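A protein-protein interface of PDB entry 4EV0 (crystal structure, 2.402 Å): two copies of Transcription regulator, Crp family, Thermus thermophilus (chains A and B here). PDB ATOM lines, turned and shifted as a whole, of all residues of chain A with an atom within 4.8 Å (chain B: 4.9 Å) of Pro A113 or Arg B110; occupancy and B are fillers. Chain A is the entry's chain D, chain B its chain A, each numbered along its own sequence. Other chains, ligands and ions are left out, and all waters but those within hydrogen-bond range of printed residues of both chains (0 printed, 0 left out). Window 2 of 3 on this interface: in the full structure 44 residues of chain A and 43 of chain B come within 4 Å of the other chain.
Of the printed residues of chain B, Ile A109 touches Pro B113. Arg A111 touches none of the printed residues of chain B. Of chain B, only Ile B109 (3.2 Å), Arg B110 (3.9 Å) and Pro B113 (3.97 Å) come within 4 Å of Pro A113. Of chain A, only Pro A113 comes within 4 Å of Arg B110. Arg B111 touches none of the printed residues of chain A. Of the printed residues of chain A, Pro B113 touches Ile A109 and Pro A113. Of the printed residues of chain A, Ala B116 touches Ala A116 (3.8 Å).
Among the printed residues, merely in contact across the chains: Pro A113 with Ile B109, Ile A109 with Pro B113, His A117 with Ile B109, Ala A116 with Ala B116, Pro A113 with Arg B110 and Pro A113 with Pro B113.
Ile A109 touches Pro B113, and with the chains exchanged Pro A113 touches Ile B109. Pro B113 touches its own counterpart, Pro A113. Ala A116 touches its own counterpart, Ala B116. 5 positions are printed for both chains. Of the 6 pairs that touch across the chains among the printed residues, 4 have their exchanged pair printed and touching as well.
Of the 9 printed residues of chain B, 4 touch a printed residue of chain A. Among the printed residues, 6 pairs touch across the chains. Among the printed residues, no Asp or Glu carboxylate lies within 4 Å of a Lys or Arg side-chain nitrogen of the other chain.
O of Leu B106 sits at hydrogen-bond distance from NH1 of Arg B110, at 2.9 Å.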
ATOM      1  N   ILE A 109       3.167 -32.625 -11.472  1.00  0.00           N
ATOM      2  CA  ILE A 109       3.668 -31.743 -12.528  1.00  0.00           C
ATOM      3  C   ILE A 109       2.569 -30.831 -13.066  1.00  0.00           C
ATOM      4  O   ILE A 109       2.859 -29.764 -13.597  1.00  0.00           O
ATOM      5  CB  ILE A 109       4.366 -32.507 -13.672  1.00  0.00           C
ATOM      6  CG1 ILE A 109       3.379 -33.387 -14.429  1.00  0.00           C
ATOM      7  CG2 ILE A 109       5.526 -33.333 -13.123  1.00  0.00           C
ATOM      8  CD1 ILE A 109       3.953 -33.960 -15.692  1.00  0.00           C
ATOM      9  N   ARG A 111       0.554 -29.265 -11.173  1.00  0.00           N
ATOM     10  CA  ARG A 111       0.702 -28.113 -10.294  1.00  0.00           C
ATOM     11  C   ARG A 111       2.079 -27.437 -10.419  1.00  0.00           C
ATOM     12  O   ARG A 111       2.162 -26.211 -10.344  1.00  0.00           O
ATOM     13  CB  ARG A 111       0.404 -28.488  -8.834  1.00  0.00           C
ATOM     14  CG  ARG A 111      -1.098 -28.540  -8.516  1.00  0.00           C
ATOM     15  CD  ARG A 111      -1.478 -27.603  -7.375  1.00  0.00           C
ATOM     16  NE  ARG A 111      -1.192 -28.205  -6.076  1.00  0.00           N
ATOM     17  CZ  ARG A 111      -1.600 -27.710  -4.908  1.00  0.00           C
ATOM     18  NH1 ARG A 111      -2.318 -26.593  -4.865  1.00  0.00           N
ATOM     19  NH2 ARG A 111      -1.293 -28.337  -3.777  1.00  0.00           N
ATOM     20  N   LEU A 112       3.144 -28.226 -10.612  1.00  0.00           N
ATOM     21  CA  LEU A 112       4.499 -27.672 -10.772  1.00  0.00           C
ATOM     22  C   LEU A 112       5.287 -28.239 -11.961  1.00  0.00           C
ATOM     23  O   LEU A 112       6.145 -29.108 -11.773  1.00  0.00           O
ATOM     24  CB  LEU A 112       5.328 -27.860  -9.493  1.00  0.00           C
ATOM     25  CG  LEU A 112       4.799 -27.173  -8.233  1.00  0.00           C
ATOM     26  CD1 LEU A 112       5.657 -27.510  -6.996  1.00  0.00           C
ATOM     27  CD2 LEU A 112       4.699 -25.664  -8.466  1.00  0.00           C
ATOM     28  N   PRO A 113       5.021 -27.724 -13.173  1.00  0.00           N
ATOM     29  CA  PRO A 113       5.653 -28.217 -14.405  1.00  0.00           C
ATOM     30  C   PRO A 113       7.175 -28.210 -14.294  1.00  0.00           C
ATOM     31  O   PRO A 113       7.869 -29.028 -14.908  1.00  0.00           O
ATOM     32  CB  PRO A 113       5.209 -27.191 -15.465  1.00  0.00           C
ATOM     33  CG  PRO A 113       4.009 -26.540 -14.922  1.00  0.00           C
ATOM     34  CD  PRO A 113       4.167 -26.547 -13.420  1.00  0.00           C
ATOM     35  N   LEU A 114       7.691 -27.283 -13.497  1.00  0.00           N
ATOM     36  CA  LEU A 114       9.125 -27.122 -13.337  1.00  0.00           C
ATOM     37  C   LEU A 114       9.795 -28.397 -12.793  1.00  0.00           C
ATOM     38  O   LEU A 114      11.028 -28.568 -12.905  1.00  0.00           O
ATOM     39  CB  LEU A 114       9.422 -25.919 -12.441  1.00  0.00           C
ATOM     40  CG  LEU A 114      10.810 -25.290 -12.579  1.00  0.00           C
ATOM     41  CD1 LEU A 114      11.059 -24.823 -14.030  1.00  0.00           C
ATOM     42  CD2 LEU A 114      10.995 -24.147 -11.581  1.00  0.00           C
ATOM     43  N   VAL A 115       8.986 -29.290 -12.218  1.00  0.00           N
ATOM     44  CA  VAL A 115       9.486 -30.586 -11.765  1.00  0.00           C
ATOM     45  C   VAL A 115       9.767 -31.494 -12.951  1.00  0.00           C
ATOM     46  O   VAL A 115      10.780 -32.181 -12.983  1.00  0.00           O
ATOM     47  CB  VAL A 115       8.494 -31.295 -10.822  1.00  0.00           C
ATOM     48  CG1 VAL A 115       8.979 -32.706 -10.509  1.00  0.00           C
ATOM     49  CG2 VAL A 115       8.314 -30.488  -9.549  1.00  0.00           C
ATOM     50  N   ALA A 116       8.863 -31.499 -13.921  1.00  0.00           N
ATOM     51  CA  ALA A 116       9.079 -32.277 -15.127  1.00  0.00           C
ATOM     52  C   ALA A 116      10.296 -31.745 -15.874  1.00  0.00           C
ATOM     53  O   ALA A 116      11.134 -32.523 -16.328  1.00  0.00           O
ATOM     54  CB  ALA A 116       7.850 -32.241 -16.019  1.00  0.00           C
ATOM     55  N   HIS A 117      10.391 -30.421 -15.996  1.00  0.00           N
ATOM     56  CA  HIS A 117      11.529 -29.801 -16.665  1.00  0.00           C
ATOM     57  C   HIS A 117      12.834 -30.125 -15.964  1.00  0.00           C
ATOM     58  O   HIS A 117      13.845 -30.381 -16.619  1.00  0.00           O
ATOM     59  CB  HIS A 117      11.385 -28.288 -16.733  1.00  0.00           C
ATOM     60  CG  HIS A 117      12.685 -27.580 -16.964  1.00  0.00           C
ATOM     61  ND1 HIS A 117      13.196 -27.346 -18.228  1.00  0.00           N
ATOM     62  CD2 HIS A 117      13.589 -27.070 -16.092  1.00  0.00           C
ATOM     63  CE1 HIS A 117      14.348 -26.710 -18.119  1.00  0.00           C
ATOM     64  NE2 HIS A 117      14.607 -26.527 -16.835  1.00  0.00           N
ATOM     65  N   LEU B 106       9.568 -22.429 -21.851  1.00  0.00           N
ATOM     66  CA  LEU B 106       9.234 -22.266 -20.446  1.00  0.00           C
ATOM     67  C   LEU B 106       7.784 -21.838 -20.259  1.00  0.00           C
ATOM     68  O   LEU B 106       7.125 -22.278 -19.315  1.00  0.00           O
ATOM     69  CB  LEU B 106      10.171 -21.260 -19.775  1.00  0.00           C
ATOM     70  CG  LEU B 106      11.538 -21.840 -19.432  1.00  0.00           C
ATOM     71  CD1 LEU B 106      12.457 -20.783 -18.811  1.00  0.00           C
ATOM     72  CD2 LEU B 106      11.340 -23.018 -18.498  1.00  0.00           C
ATOM     73  N   ALA B 107       7.292 -20.979 -21.152  1.00  0.00           N
ATOM     74  CA  ALA B 107       5.910 -20.534 -21.071  1.00  0.00           C
ATOM     75  C   ALA B 107       4.978 -21.684 -21.441  1.00  0.00           C
ATOM     76  O   ALA B 107       3.903 -21.839 -20.860  1.00  0.00           O
ATOM     77  CB  ALA B 107       5.674 -19.340 -21.977  1.00  0.00           C
ATOM     78  N   LEU B 108       5.406 -22.500 -22.400  1.00  0.00           N
ATOM     79  CA  LEU B 108       4.566 -23.562 -22.930  1.00  0.00           C
ATOM     80  C   LEU B 108       4.308 -24.685 -21.904  1.00  0.00           C
ATOM     81  O   LEU B 108       3.148 -25.098 -21.678  1.00  0.00           O
ATOM     82  CB  LEU B 108       5.189 -24.132 -24.197  1.00  0.00           C
ATOM     83  CG  LEU B 108       4.594 -25.427 -24.744  1.00  0.00           C
ATOM     84  CD1 LEU B 108       3.127 -25.240 -25.111  1.00  0.00           C
ATOM     85  CD2 LEU B 108       5.418 -25.919 -25.943  1.00  0.00           C
ATOM     86  N   ILE B 109       5.372 -25.174 -21.278  1.00  0.00           N
ATOM     87  CA  ILE B 109       5.203 -26.249 -20.319  1.00  0.00           C
ATOM     88  C   ILE B 109       4.444 -25.766 -19.076  1.00  0.00           C
ATOM     89  O   ILE B 109       3.874 -26.564 -18.344  1.00  0.00           O
ATOM     90  CB  ILE B 109       6.548 -26.894 -19.933  1.00  0.00           C
ATOM     91  CG1 ILE B 109       7.291 -26.041 -18.900  1.00  0.00           C
ATOM     92  CG2 ILE B 109       7.396 -27.126 -21.186  1.00  0.00           C
ATOM     93  CD1 ILE B 109       8.572 -26.687 -18.378  1.00  0.00           C
ATOM     94  N   ARG B 110       4.440 -24.457 -18.854  1.00  0.00           N
ATOM     95  CA  ARG B 110       3.676 -23.861 -17.774  1.00  0.00           C
ATOM     96  C   ARG B 110       2.181 -24.015 -18.089  1.00  0.00           C
ATOM     97  O   ARG B 110       1.341 -24.102 -17.199  1.00  0.00           O
ATOM     98  CB  ARG B 110       4.058 -22.386 -17.649  1.00  0.00           C
ATOM     99  CG  ARG B 110       3.643 -21.716 -16.353  1.00  0.00           C
ATOM    100  CD  ARG B 110       4.788 -20.856 -15.813  1.00  0.00           C
ATOM    101  NE  ARG B 110       5.983 -21.658 -15.537  1.00  0.00           N
ATOM    102  CZ  ARG B 110       7.164 -21.468 -16.117  1.00  0.00           C
ATOM    103  NH1 ARG B 110       7.311 -20.493 -17.009  1.00  0.00           N
ATOM    104  NH2 ARG B 110       8.199 -22.252 -15.813  1.00  0.00           N
ATOM    105  N   ARG B 111       1.890 -24.087 -19.385  1.00  0.00           N
ATOM    106  CA  ARG B 111       0.533 -24.178 -19.904  1.00  0.00           C
ATOM    107  C   ARG B 111       0.170 -25.626 -20.256  1.00  0.00           C
ATOM    108  O   ARG B 111      -0.974 -26.025 -20.140  1.00  0.00           O
ATOM    109  CB  ARG B 111       0.426 -23.278 -21.145  1.00  0.00           C
ATOM    110  CG  ARG B 111      -0.923 -23.241 -21.822  1.00  0.00           C
ATOM    111  CD  ARG B 111      -1.970 -22.539 -20.968  1.00  0.00           C
ATOM    112  NE  ARG B 111      -3.277 -22.573 -21.617  1.00  0.00           N
ATOM    113  CZ  ARG B 111      -4.092 -23.618 -21.581  1.00  0.00           C
ATOM    114  NH1 ARG B 111      -3.735 -24.715 -20.922  1.00  0.00           N
ATOM    115  NH2 ARG B 111      -5.262 -23.567 -22.208  1.00  0.00           N
ATOM    116  N   LEU B 112       1.164 -26.402 -20.706  1.00  0.00           N
ATOM    117  CA  LEU B 112       0.982 -27.826 -21.032  1.00  0.00           C
ATOM    118  C   LEU B 112       2.112 -28.684 -20.455  1.00  0.00           C
ATOM    119  O   LEU B 112       3.053 -29.082 -21.169  1.00  0.00           O
ATOM    120  CB  LEU B 112       0.860 -28.033 -22.540  1.00  0.00           C
ATOM    121  CG  LEU B 112      -0.398 -27.393 -23.137  1.00  0.00           C
ATOM    122  CD1 LEU B 112      -0.341 -27.444 -24.656  1.00  0.00           C
ATOM    123  CD2 LEU B 112      -1.675 -28.060 -22.598  1.00  0.00           C
ATOM    124  N   PRO B 113       2.023 -28.979 -19.151  1.00  0.00           N
ATOM    125  CA  PRO B 113       3.081 -29.700 -18.420  1.00  0.00           C
ATOM    126  C   PRO B 113       3.489 -31.026 -19.077  1.00  0.00           C
ATOM    127  O   PRO B 113       4.652 -31.417 -18.998  1.00  0.00           O
ATOM    128  CB  PRO B 113       2.451 -29.943 -17.046  1.00  0.00           C
ATOM    129  CG  PRO B 113       1.442 -28.836 -16.895  1.00  0.00           C
ATOM    130  CD  PRO B 113       0.898 -28.600 -18.280  1.00  0.00           C
ATOM    131  N   ALA B 116       6.640 -31.025 -21.124  1.00  0.00           N
ATOM    132  CA  ALA B 116       7.907 -31.149 -20.431  1.00  0.00           C
ATOM    133  C   ALA B 116       8.129 -32.618 -20.047  1.00  0.00           C
ATOM    134  O   ALA B 116       9.237 -33.140 -20.200  1.00  0.00           O
ATOM    135  CB  ALA B 116       7.949 -30.243 -19.217  1.00  0.00           C
